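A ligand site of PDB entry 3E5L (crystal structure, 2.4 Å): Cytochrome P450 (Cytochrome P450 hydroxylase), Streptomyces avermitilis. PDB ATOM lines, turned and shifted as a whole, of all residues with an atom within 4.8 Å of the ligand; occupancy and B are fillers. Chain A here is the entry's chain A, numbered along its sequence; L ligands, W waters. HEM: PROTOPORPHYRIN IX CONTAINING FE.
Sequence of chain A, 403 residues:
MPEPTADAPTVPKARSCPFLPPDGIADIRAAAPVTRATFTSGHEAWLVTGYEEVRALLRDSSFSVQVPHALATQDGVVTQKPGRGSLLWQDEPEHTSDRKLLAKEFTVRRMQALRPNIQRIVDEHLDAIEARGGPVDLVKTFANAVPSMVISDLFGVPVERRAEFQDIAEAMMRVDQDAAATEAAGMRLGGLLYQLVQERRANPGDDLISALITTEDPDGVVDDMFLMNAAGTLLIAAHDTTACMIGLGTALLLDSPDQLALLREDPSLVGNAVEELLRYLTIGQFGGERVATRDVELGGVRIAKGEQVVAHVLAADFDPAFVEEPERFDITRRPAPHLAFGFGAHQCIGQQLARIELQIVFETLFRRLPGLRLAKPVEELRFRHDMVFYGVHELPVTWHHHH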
ATOM      1  N   LEU A  87      12.887  -4.950 -24.869  1.00  0.00           N
ATOM      2  CA  LEU A  87      13.618  -4.283 -23.771  1.00  0.00           C
ATOM      3  C   LEU A  87      13.896  -2.800 -23.954  1.00  0.00           C
ATOM      4  O   LEU A  87      13.641  -2.032 -23.052  1.00  0.00           O
ATOM      5  CB  LEU A  87      14.928  -4.982 -23.427  1.00  0.00           C
ATOM      6  CG  LEU A  87      14.898  -6.454 -22.960  1.00  0.00           C
ATOM      7  CD1 LEU A  87      16.248  -6.820 -22.253  1.00  0.00           C
ATOM      8  CD2 LEU A  87      13.675  -6.735 -22.025  1.00  0.00           C
ATOM      9  N   LEU A  88      14.448  -2.428 -25.104  1.00  0.00           N
ATOM     10  CA  LEU A  88      15.028  -1.099 -25.347  1.00  0.00           C
ATOM     11  C   LEU A  88      14.041   0.039 -25.114  1.00  0.00           C
ATOM     12  O   LEU A  88      14.378   1.088 -24.551  1.00  0.00           O
ATOM     13  CB  LEU A  88      15.441  -1.041 -26.807  1.00  0.00           C
ATOM     14  CG  LEU A  88      16.947  -1.012 -27.133  1.00  0.00           C
ATOM     15  CD1 LEU A  88      17.849  -0.514 -25.899  1.00  0.00           C
ATOM     16  CD2 LEU A  88      17.436  -2.295 -27.751  1.00  0.00           C
ATOM     17  N   HIS A  95       9.305  -3.835 -18.908  1.00  0.00           N
ATOM     18  CA  HIS A  95      10.766  -3.964 -18.939  1.00  0.00           C
ATOM     19  C   HIS A  95      11.088  -4.514 -17.568  1.00  0.00           C
ATOM     20  O   HIS A  95      10.420  -4.192 -16.630  1.00  0.00           O
ATOM     21  CB  HIS A  95      11.414  -2.593 -19.054  1.00  0.00           C
ATOM     22  CG  HIS A  95      12.905  -2.652 -19.010  1.00  0.00           C
ATOM     23  ND1 HIS A  95      13.619  -2.517 -17.839  1.00  0.00           N
ATOM     24  CD2 HIS A  95      13.816  -2.948 -19.985  1.00  0.00           C
ATOM     25  CE1 HIS A  95      14.907  -2.694 -18.096  1.00  0.00           C
ATOM     26  NE2 HIS A  95      15.046  -2.947 -19.386  1.00  0.00           N
ATOM     27  N   ARG A  99      12.950  -8.315 -18.914  1.00  0.00           N
ATOM     28  CA  ARG A  99      14.396  -8.409 -18.809  1.00  0.00           C
ATOM     29  C   ARG A  99      14.791  -9.564 -17.894  1.00  0.00           C
ATOM     30  O   ARG A  99      15.663 -10.352 -18.222  1.00  0.00           O
ATOM     31  CB  ARG A  99      14.999  -7.108 -18.326  1.00  0.00           C
ATOM     32  CG  ARG A  99      16.463  -7.225 -18.205  1.00  0.00           C
ATOM     33  CD  ARG A  99      17.196  -5.922 -18.275  1.00  0.00           C
ATOM     34  NE  ARG A  99      18.583  -6.142 -17.852  1.00  0.00           N
ATOM     35  CZ  ARG A  99      19.617  -5.423 -18.263  1.00  0.00           C
ATOM     36  NH1 ARG A  99      19.465  -4.427 -19.165  1.00  0.00           N
ATOM     37  NH2 ARG A  99      20.812  -5.714 -17.798  1.00  0.00           N
ATOM     38  N   PHE A 106      19.729 -16.009 -20.730  1.00  0.00           N
ATOM     39  CA  PHE A 106      20.900 -15.253 -21.247  1.00  0.00           C
ATOM     40  C   PHE A 106      21.731 -14.811 -20.056  1.00  0.00           C
ATOM     41  O   PHE A 106      21.700 -13.659 -19.651  1.00  0.00           O
ATOM     42  CB  PHE A 106      20.446 -14.049 -22.088  1.00  0.00           C
ATOM     43  CG  PHE A 106      21.580 -13.389 -22.831  1.00  0.00           C
ATOM     44  CD1 PHE A 106      21.766 -12.009 -22.787  1.00  0.00           C
ATOM     45  CD2 PHE A 106      22.546 -14.169 -23.483  1.00  0.00           C
ATOM     46  CE1 PHE A 106      22.869 -11.441 -23.408  1.00  0.00           C
ATOM     47  CE2 PHE A 106      23.630 -13.603 -24.128  1.00  0.00           C
ATOM     48  CZ  PHE A 106      23.791 -12.235 -24.096  1.00  0.00           C
ATOM     49  N   ILE A 151      26.533 -14.223 -32.308  1.00  0.00           N
ATOM     50  CA  ILE A 151      25.092 -14.270 -32.020  1.00  0.00           C
ATOM     51  C   ILE A 151      24.448 -15.535 -32.670  1.00  0.00           C
ATOM     52  O   ILE A 151      23.612 -16.210 -32.040  1.00  0.00           O
ATOM     53  CB  ILE A 151      24.402 -12.951 -32.446  1.00  0.00           C
ATOM     54  CG1 ILE A 151      24.961 -11.763 -31.613  1.00  0.00           C
ATOM     55  CG2 ILE A 151      22.910 -13.080 -32.306  1.00  0.00           C
ATOM     56  CD1 ILE A 151      24.749 -11.947 -30.069  1.00  0.00           C
ATOM     57  N   LEU A 154      24.968 -18.323 -30.395  1.00  0.00           N
ATOM     58  CA  LEU A 154      24.133 -18.131 -29.227  1.00  0.00           C
ATOM     59  C   LEU A 154      22.736 -18.702 -29.525  1.00  0.00           C
ATOM     60  O   LEU A 154      22.062 -19.301 -28.666  1.00  0.00           O
ATOM     61  CB  LEU A 154      24.057 -16.625 -28.866  1.00  0.00           C
ATOM     62  CG  LEU A 154      23.211 -16.153 -27.693  1.00  0.00           C
ATOM     63  CD1 LEU A 154      23.784 -16.731 -26.370  1.00  0.00           C
ATOM     64  CD2 LEU A 154      23.138 -14.567 -27.570  1.00  0.00           C
ATOM     65  N   THR A 233      16.422  -8.032 -31.004  1.00  0.00           N
ATOM     66  CA  THR A 233      17.080  -7.010 -30.200  1.00  0.00           C
ATOM     67  C   THR A 233      18.490  -7.448 -29.821  1.00  0.00           C
ATOM     68  O   THR A 233      19.433  -6.653 -29.930  1.00  0.00           O
ATOM     69  CB  THR A 233      16.212  -6.701 -28.944  1.00  0.00           C
ATOM     70  OG1 THR A 233      15.045  -6.032 -29.414  1.00  0.00           O
ATOM     71  CG2 THR A 233      16.881  -5.769 -28.021  1.00  0.00           C
ATOM     72  N   LEU A 234      18.638  -8.701 -29.391  1.00  0.00           N
ATOM     73  CA  LEU A 234      19.955  -9.248 -29.060  1.00  0.00           C
ATOM     74  C   LEU A 234      20.871  -9.143 -30.242  1.00  0.00           C
ATOM     75  O   LEU A 234      22.005  -8.628 -30.111  1.00  0.00           O
ATOM     76  CB  LEU A 234      19.878 -10.707 -28.602  1.00  0.00           C
ATOM     77  CG  LEU A 234      19.239 -10.862 -27.214  1.00  0.00           C
ATOM     78  CD1 LEU A 234      18.993 -12.330 -26.864  1.00  0.00           C
ATOM     79  CD2 LEU A 234      20.109 -10.158 -26.130  1.00  0.00           C
ATOM     80  N   ALA A 237      21.470  -5.245 -31.181  1.00  0.00           N
ATOM     81  CA  ALA A 237      22.210  -4.555 -30.147  1.00  0.00           C
ATOM     82  C   ALA A 237      23.664  -5.073 -30.106  1.00  0.00           C
ATOM     83  O   ALA A 237      24.545  -4.338 -29.693  1.00  0.00           O
ATOM     84  CB  ALA A 237      21.499  -4.740 -28.775  1.00  0.00           C
ATOM     85  N   ALA A 238      23.872  -6.324 -30.508  1.00  0.00           N
ATOM     86  CA  ALA A 238      25.159  -7.004 -30.335  1.00  0.00           C
ATOM     87  C   ALA A 238      26.084  -6.809 -31.520  1.00  0.00           C
ATOM     88  O   ALA A 238      27.278  -7.041 -31.382  1.00  0.00           O
ATOM     89  CB  ALA A 238      24.947  -8.512 -30.178  1.00  0.00           C
ATOM     90  N   THR A 241      27.411  -2.466 -32.526  1.00  0.00           N
ATOM     91  CA  THR A 241      28.217  -2.026 -31.400  1.00  0.00           C
ATOM     92  C   THR A 241      29.601  -2.779 -31.374  1.00  0.00           C
ATOM     93  O   THR A 241      30.627  -2.166 -31.512  1.00  0.00           O
ATOM     94  CB  THR A 241      27.454  -2.286 -30.086  1.00  0.00           C
ATOM     95  OG1 THR A 241      26.953  -3.641 -30.093  1.00  0.00           O
ATOM     96  CG2 THR A 241      26.311  -1.364 -29.937  1.00  0.00           C
ATOM     97  N   THR A 242      29.611  -4.097 -31.263  1.00  0.00           N
ATOM     98  CA  THR A 242      30.852  -4.869 -31.237  1.00  0.00           C
ATOM     99  C   THR A 242      31.667  -4.597 -32.482  1.00  0.00           C
ATOM    100  O   THR A 242      32.887  -4.358 -32.365  1.00  0.00           O
ATOM    101  CB  THR A 242      30.524  -6.355 -31.082  1.00  0.00           C
ATOM    102  OG1 THR A 242      29.599  -6.496 -29.998  1.00  0.00           O
ATOM    103  CG2 THR A 242      31.754  -7.187 -30.719  1.00  0.00           C
ATOM    104  N   MET A 245      33.383  -1.325 -32.177  1.00  0.00           N
ATOM    105  CA  MET A 245      34.510  -1.408 -31.295  1.00  0.00           C
ATOM    106  C   MET A 245      35.704  -2.144 -31.918  1.00  0.00           C
ATOM    107  O   MET A 245      36.862  -1.772 -31.688  1.00  0.00           O
ATOM    108  CB  MET A 245      34.156  -2.074 -29.932  1.00  0.00           C
ATOM    109  CG  MET A 245      33.360  -1.193 -29.002  1.00  0.00           C
ATOM    110  SD  MET A 245      34.225   0.341 -28.586  1.00  0.00           S
ATOM    111  CE  MET A 245      35.736  -0.390 -27.876  1.00  0.00           C
ATOM    112  N   LEU A 278      36.989   0.860 -24.532  1.00  0.00           N
ATOM    113  CA  LEU A 278      35.584   1.122 -24.288  1.00  0.00           C
ATOM    114  C   LEU A 278      35.407   2.540 -23.764  1.00  0.00           C
ATOM    115  O   LEU A 278      34.578   3.242 -24.298  1.00  0.00           O
ATOM    116  CB  LEU A 278      34.939   0.113 -23.317  1.00  0.00           C
ATOM    117  CG  LEU A 278      34.819  -1.257 -23.968  1.00  0.00           C
ATOM    118  CD1 LEU A 278      34.669  -2.329 -22.866  1.00  0.00           C
ATOM    119  CD2 LEU A 278      33.562  -1.255 -24.960  1.00  0.00           C
ATOM    120  N   ILE A 283      31.320   4.479 -27.893  1.00  0.00           N
ATOM    121  CA  ILE A 283      30.781   4.479 -29.282  1.00  0.00           C
ATOM    122  C   ILE A 283      29.330   4.964 -29.430  1.00  0.00           C
ATOM    123  O   ILE A 283      28.949   5.523 -30.463  1.00  0.00           O
ATOM    124  CB  ILE A 283      31.024   3.077 -29.992  1.00  0.00           C
ATOM    125  CG1 ILE A 283      30.377   1.927 -29.215  1.00  0.00           C
ATOM    126  CG2 ILE A 283      32.525   2.860 -30.290  1.00  0.00           C
ATOM    127  CD1 ILE A 283      30.154   0.676 -30.045  1.00  0.00           C
ATOM    128  N   GLY A 288      22.341   8.270 -24.052  1.00  0.00           N
ATOM    129  CA  GLY A 288      21.012   7.696 -23.733  1.00  0.00           C
ATOM    130  C   GLY A 288      19.929   8.752 -23.615  1.00  0.00           C
ATOM    131  O   GLY A 288      20.122   9.813 -22.955  1.00  0.00           O
ATOM    132  N   ARG A 290      16.295  10.022 -22.272  1.00  0.00           N
ATOM    133  CA  ARG A 290      15.260   9.720 -21.293  1.00  0.00           C
ATOM    134  C   ARG A 290      14.274  10.868 -21.215  1.00  0.00           C
ATOM    135  O   ARG A 290      14.571  11.980 -21.684  1.00  0.00           O
ATOM    136  CB  ARG A 290      15.881   9.423 -19.904  1.00  0.00           C
ATOM    137  CG  ARG A 290      17.028   8.395 -19.903  1.00  0.00           C
ATOM    138  CD  ARG A 290      16.460   6.976 -20.187  1.00  0.00           C
ATOM    139  NE  ARG A 290      17.345   5.873 -19.847  1.00  0.00           N
ATOM    140  CZ  ARG A 290      18.232   5.379 -20.691  1.00  0.00           C
ATOM    141  NH1 ARG A 290      18.344   5.880 -21.912  1.00  0.00           N
ATOM    142  NH2 ARG A 290      18.994   4.365 -20.334  1.00  0.00           N
ATOM    143  N   ALA A 340      30.418   3.132 -21.095  1.00  0.00           N
ATOM    144  CA  ALA A 340      30.213   2.612 -22.439  1.00  0.00           C
ATOM    145  C   ALA A 340      29.057   1.622 -22.569  1.00  0.00           C
ATOM    146  O   ALA A 340      28.591   1.386 -23.673  1.00  0.00           O
ATOM    147  CB  ALA A 340      31.465   1.965 -22.902  1.00  0.00           C
ATOM    148  N   PHE A 341      28.667   0.951 -21.468  1.00  0.00           N
ATOM    149  CA  PHE A 341      27.599  -0.059 -21.539  1.00  0.00           C
ATOM    150  C   PHE A 341      26.338   0.519 -20.830  1.00  0.00           C
ATOM    151  O   PHE A 341      25.387  -0.211 -20.559  1.00  0.00           O
ATOM    152  CB  PHE A 341      28.023  -1.341 -20.855  1.00  0.00           C
ATOM    153  CG  PHE A 341      29.043  -2.148 -21.617  1.00  0.00           C
ATOM    154  CD1 PHE A 341      28.759  -2.648 -22.885  1.00  0.00           C
ATOM    155  CD2 PHE A 341      30.296  -2.389 -21.069  1.00  0.00           C
ATOM    156  CE1 PHE A 341      29.693  -3.356 -23.595  1.00  0.00           C
ATOM    157  CE2 PHE A 341      31.279  -3.112 -21.779  1.00  0.00           C
ATOM    158  CZ  PHE A 341      30.983  -3.583 -23.043  1.00  0.00           C
ATOM    159  N   GLY A 342      26.394   1.799 -20.483  1.00  0.00           N
ATOM    160  CA  GLY A 342      25.237   2.414 -19.876  1.00  0.00           C
ATOM    161  C   GLY A 342      25.305   2.108 -18.411  1.00  0.00           C
ATOM    162  O   GLY A 342      26.370   1.755 -17.916  1.00  0.00           O
ATOM    163  N   ALA A 345      18.954   0.375 -15.034  1.00  0.00           N
ATOM    164  CA  ALA A 345      18.086  -0.759 -15.453  1.00  0.00           C
ATOM    165  C   ALA A 345      18.240  -1.144 -16.925  1.00  0.00           C
ATOM    166  O   ALA A 345      17.984  -2.291 -17.275  1.00  0.00           O
ATOM    167  CB  ALA A 345      16.690  -0.408 -15.212  1.00  0.00           C
ATOM    168  N   HIS A 346      18.656  -0.214 -17.777  1.00  0.00           N
ATOM    169  CA  HIS A 346      18.778  -0.525 -19.204  1.00  0.00           C
ATOM    170  C   HIS A 346      20.210  -0.826 -19.571  1.00  0.00           C
ATOM    171  O   HIS A 346      20.521  -0.944 -20.723  1.00  0.00           O
ATOM    172  CB  HIS A 346      18.206   0.581 -20.100  1.00  0.00           C
ATOM    173  CG  HIS A 346      16.693   0.623 -20.084  1.00  0.00           C
ATOM    174  ND1 HIS A 346      15.922  -0.146 -20.936  1.00  0.00           N
ATOM    175  CD2 HIS A 346      15.833   1.282 -19.272  1.00  0.00           C
ATOM    176  CE1 HIS A 346      14.641   0.068 -20.664  1.00  0.00           C
ATOM    177  NE2 HIS A 346      14.566   0.924 -19.654  1.00  0.00           N
ATOM    178  N   GLN A 347      21.083  -0.970 -18.597  1.00  0.00           N
ATOM    179  CA  GLN A 347      22.450  -1.167 -18.930  1.00  0.00           C
ATOM    180  C   GLN A 347      22.704  -2.434 -19.732  1.00  0.00           C
ATOM    181  O   GLN A 347      22.086  -3.463 -19.492  1.00  0.00           O
ATOM    182  CB  GLN A 347      23.294  -1.085 -17.669  1.00  0.00           C
ATOM    183  CG  GLN A 347      23.809  -2.289 -17.126  1.00  0.00           C
ATOM    184  CD  GLN A 347      24.854  -1.951 -16.068  1.00  0.00           C
ATOM    185  OE1 GLN A 347      26.017  -1.541 -16.367  1.00  0.00           O
ATOM    186  NE2 GLN A 347      24.402  -2.000 -14.800  1.00  0.00           N
ATOM    187  N   CYS A 348      23.647  -2.350 -20.660  1.00  0.00           N
ATOM    188  CA  CYS A 348      23.848  -3.422 -21.573  1.00  0.00           C
ATOM    189  C   CYS A 348      23.772  -4.782 -20.865  1.00  0.00           C
ATOM    190  O   CYS A 348      24.559  -5.079 -19.952  1.00  0.00           O
ATOM    191  CB  CYS A 348      25.164  -3.275 -22.287  1.00  0.00           C
ATOM    192  SG  CYS A 348      25.348  -4.578 -23.433  1.00  0.00           S
ATOM    193  N   ILE A 349      22.836  -5.620 -21.312  1.00  0.00           N
ATOM    194  CA  ILE A 349      22.716  -6.989 -20.773  1.00  0.00           C
ATOM    195  C   ILE A 349      23.780  -7.958 -21.349  1.00  0.00           C
ATOM    196  O   ILE A 349      24.047  -9.002 -20.758  1.00  0.00           O
ATOM    197  CB  ILE A 349      21.237  -7.556 -21.013  1.00  0.00           C
ATOM    198  CG1 ILE A 349      20.917  -8.747 -20.124  1.00  0.00           C
ATOM    199  CG2 ILE A 349      20.960  -7.876 -22.514  1.00  0.00           C
ATOM    200  CD1 ILE A 349      19.424  -9.222 -20.371  1.00  0.00           C
ATOM    201  N   GLY A 350      24.374  -7.612 -22.488  1.00  0.00           N
ATOM    202  CA  GLY A 350      25.307  -8.502 -23.138  1.00  0.00           C
ATOM    203  C   GLY A 350      26.728  -8.082 -22.925  1.00  0.00           C
ATOM    204  O   GLY A 350      27.618  -8.565 -23.627  1.00  0.00           O
ATOM    205  N   LEU A 353      29.450 -10.620 -22.551  1.00  0.00           N
ATOM    206  CA  LEU A 353      29.724 -11.225 -23.835  1.00  0.00           C
ATOM    207  C   LEU A 353      30.589 -10.323 -24.763  1.00  0.00           C
ATOM    208  O   LEU A 353      31.539 -10.782 -25.408  1.00  0.00           O
ATOM    209  CB  LEU A 353      28.408 -11.631 -24.505  1.00  0.00           C
ATOM    210  CG  LEU A 353      28.663 -12.433 -25.812  1.00  0.00           C
ATOM    211  CD1 LEU A 353      29.548 -13.728 -25.605  1.00  0.00           C
ATOM    212  CD2 LEU A 353      27.390 -12.780 -26.484  1.00  0.00           C
ATOM    213  N   ALA A 354      30.249  -9.034 -24.810  1.00  0.00           N
ATOM    214  CA  ALA A 354      30.987  -8.084 -25.612  1.00  0.00           C
ATOM    215  C   ALA A 354      32.435  -8.024 -25.153  1.00  0.00           C
ATOM    216  O   ALA A 354      33.328  -8.029 -26.003  1.00  0.00           O
ATOM    217  CB  ALA A 354      30.340  -6.727 -25.534  1.00  0.00           C
ATOM    218  N   GLU A 357      34.169 -11.129 -26.282  1.00  0.00           N
ATOM    219  CA  GLU A 357      34.487 -11.055 -27.709  1.00  0.00           C
ATOM    220  C   GLU A 357      35.671 -10.169 -27.999  1.00  0.00           C
ATOM    221  O   GLU A 357      36.526 -10.504 -28.813  1.00  0.00           O
ATOM    222  CB  GLU A 357      33.314 -10.519 -28.579  1.00  0.00           C
ATOM    223  CG  GLU A 357      32.133 -11.430 -28.654  1.00  0.00           C
ATOM    224  CD  GLU A 357      31.131 -10.958 -29.702  1.00  0.00           C
ATOM    225  OE1 GLU A 357      30.001 -10.756 -29.291  1.00  0.00           O
ATOM    226  OE2 GLU A 357      31.469 -10.692 -30.880  1.00  0.00           O
ATOM    227  N   LEU A 358      35.706  -8.996 -27.361  1.00  0.00           N
ATOM    228  CA  LEU A 358      36.759  -8.049 -27.651  1.00  0.00           C
ATOM    229  C   LEU A 358      38.098  -8.534 -27.122  1.00  0.00           C
ATOM    230  O   LEU A 358      39.101  -8.320 -27.754  1.00  0.00           O
ATOM    231  CB  LEU A 358      36.401  -6.680 -27.057  1.00  0.00           C
ATOM    232  CG  LEU A 358      35.186  -5.986 -27.682  1.00  0.00           C
ATOM    233  CD1 LEU A 358      34.942  -4.680 -26.916  1.00  0.00           C
ATOM    234  CD2 LEU A 358      35.395  -5.744 -29.205  1.00  0.00           C
HETATM  235  CHA HEM L   1      21.623  -2.248 -23.843  1.00  0.00           C
HETATM  236  CHB HEM L   1      25.978  -0.542 -25.333  1.00  0.00           C
HETATM  237  CHC HEM L   1      27.480  -4.977 -26.994  1.00  0.00           C
HETATM  238  CHD HEM L   1      22.894  -6.510 -26.021  1.00  0.00           C
HETATM  239  C1A HEM L   1      22.757  -1.425 -24.039  1.00  0.00           C
HETATM  240  C2A HEM L   1      23.014  -0.082 -23.587  1.00  0.00           C
HETATM  241  C3A HEM L   1      24.212   0.287 -24.079  1.00  0.00           C
HETATM  242  C4A HEM L   1      24.728  -0.740 -24.764  1.00  0.00           C
HETATM  243  CMA HEM L   1      25.093   1.612 -24.098  1.00  0.00           C
HETATM  244  CAA HEM L   1      22.115   0.906 -22.793  1.00  0.00           C
HETATM  245  CBA HEM L   1      21.345   1.675 -23.861  1.00  0.00           C
HETATM  246  CGA HEM L   1      20.701   2.847 -23.097  1.00  0.00           C
HETATM  247  O1A HEM L   1      20.802   2.930 -21.843  1.00  0.00           O
HETATM  248  O2A HEM L   1      20.074   3.726 -23.749  1.00  0.00           O
HETATM  249  C1B HEM L   1      26.745  -1.636 -25.895  1.00  0.00           C
HETATM  250  C2B HEM L   1      28.130  -1.600 -26.334  1.00  0.00           C
HETATM  251  C3B HEM L   1      28.515  -2.815 -26.815  1.00  0.00           C
HETATM  252  C4B HEM L   1      27.393  -3.632 -26.660  1.00  0.00           C
HETATM  253  CMB HEM L   1      29.236  -0.473 -26.337  1.00  0.00           C
HETATM  254  CAB HEM L   1      29.998  -3.115 -27.267  1.00  0.00           C
HETATM  255  CBB HEM L   1      30.472  -4.121 -27.931  1.00  0.00           C
HETATM  256  C1C HEM L   1      26.361  -5.876 -26.774  1.00  0.00           C
HETATM  257  C2C HEM L   1      26.191  -7.352 -26.934  1.00  0.00           C
HETATM  258  C3C HEM L   1      24.864  -7.585 -26.649  1.00  0.00           C
HETATM  259  C4C HEM L   1      24.256  -6.402 -26.290  1.00  0.00           C
HETATM  260  CMC HEM L   1      27.282  -8.430 -27.364  1.00  0.00           C
HETATM  261  CAC HEM L   1      23.768  -8.745 -26.516  1.00  0.00           C
HETATM  262  CBC HEM L   1      23.997 -10.167 -26.794  1.00  0.00           C
HETATM  263  C1D HEM L   1      22.023  -5.477 -25.465  1.00  0.00           C
HETATM  264  C2D HEM L   1      20.577  -5.464 -25.147  1.00  0.00           C
HETATM  265  C3D HEM L   1      20.321  -4.129 -24.479  1.00  0.00           C
HETATM  266  C4D HEM L   1      21.556  -3.484 -24.466  1.00  0.00           C
HETATM  267  CMD HEM L   1      19.337  -6.432 -25.386  1.00  0.00           C
HETATM  268  CAD HEM L   1      19.059  -3.325 -23.878  1.00  0.00           C
HETATM  269  CBD HEM L   1      18.911  -3.697 -22.356  1.00  0.00           C
HETATM  270  CGD HEM L   1      17.717  -3.047 -21.729  1.00  0.00           C
HETATM  271  O1D HEM L   1      17.262  -3.394 -20.578  1.00  0.00           O
HETATM  272  O2D HEM L   1      17.210  -2.097 -22.353  1.00  0.00           O
HETATM  273  NA  HEM L   1      23.927  -1.821 -24.761  1.00  0.00           N
HETATM  274  NB  HEM L   1      26.285  -3.009 -26.149  1.00  0.00           N
HETATM  275  NC  HEM L   1      25.066  -5.336 -26.331  1.00  0.00           N
HETATM  276  ND  HEM L   1      22.564  -4.204 -25.008  1.00  0.00           N
HETATM  277 FE   HEM L   1      24.489  -3.638 -25.455  1.00  0.00          FE
HETATM  278  O   HOH W   1      21.875   2.594 -19.647  1.00  0.00           O
HETATM  279  O   HOH W   2      23.751  -2.557 -27.830  1.00  0.00           O
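The side-chain sulfur (SG) of Cys 348 is bound to an iron atom (FE) of the ligand. The guanidinium group of Arg 290 is in salt-bridge range of an oxygen (O1A) of the ligand, 2.8 Å away. A ring nitrogen (NE2) of His 95 is in hydrogen-bond range of an oxygen (O1D) of the ligand, at 2.6 Å. A ring nitrogen (ND1) of His 346 sits at hydrogen-bond distance from an oxygen (O2D) of the ligand, at 2.7 Å. The guanidinium group of Arg 99 lies within salt-bridge range of an oxygen (O1D) of the ligand.
Water W1 lies within hydrogen-bond range of an oxygen (O1A) of the ligand and the guanidinium group of Arg 290.
The side-chain hydroxyl of Thr 241 lies within hydrogen-bond range of the backbone carbonyl oxygen of Ala 237 (2.5 Å). The guanidinium group (NH1) of Arg 99 lies within hydrogen-bond range of the backbone carbonyl oxygen (O) of Gln 347, at 2.8 Å. A ring nitrogen (NE2) of His 95 sits close to a ring nitrogen (ND1) of His 346 (3.3 Å). The backbone carbonyl oxygen of Ala 345 is in hydrogen-bond range of the guanidinium group of Arg 99 (3.2 Å). The backbone NH (N) of Gly 350 sits close to the side-chain sulfur (SG) of Cys 348, 3.3 Å away. The backbone carbonyl oxygen of Ala 238 is in hydrogen-bond range of the side-chain hydroxyl of Thr 242 (2.8 Å). The backbone NH (N) of Cys 348 lies within hydrogen-bond range of the backbone carbonyl oxygen (O) of Phe 341 (2.8 Å).
Residues that only touch the ligand: Leu 87 (3.6 Å), Leu 88 (3.7 Å), Phe 106 (3.4 Å), Ile 151 (3.8 Å), Thr 233 (3.7 Å), Leu 234 (3.9 Å), Ala 237 (3.4 Å), Ala 238 (3.6 Å), Thr 241 (3.4 Å), Thr 242 (3.3 Å), Ile 283 (3.9 Å), Ala 340 (3.3 Å), Phe 341 (3.5 Å), Gly 342 (3.8 Å), Ala 345 (3.6 Å), Ile 349 (3.6 Å), Gly 350 (3.7 Å) and Ala 354 (3.5 Å). 23 residues have an atom within 4 Å of the ligand: Leu 87, Leu 88, His 95, Arg 99, Phe 106, Ile 151, Thr 233, Leu 234, Ala 237, Ala 238, Thr 241, Thr 242, Ile 283, Arg 290, Ala 340, Phe 341, Gly 342, Ala 345, His 346, Cys 348, Ile 349, Gly 350 and Ala 354. The nearest printed residue that does not touch the ligand is Glu 357 (4.1 Å).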
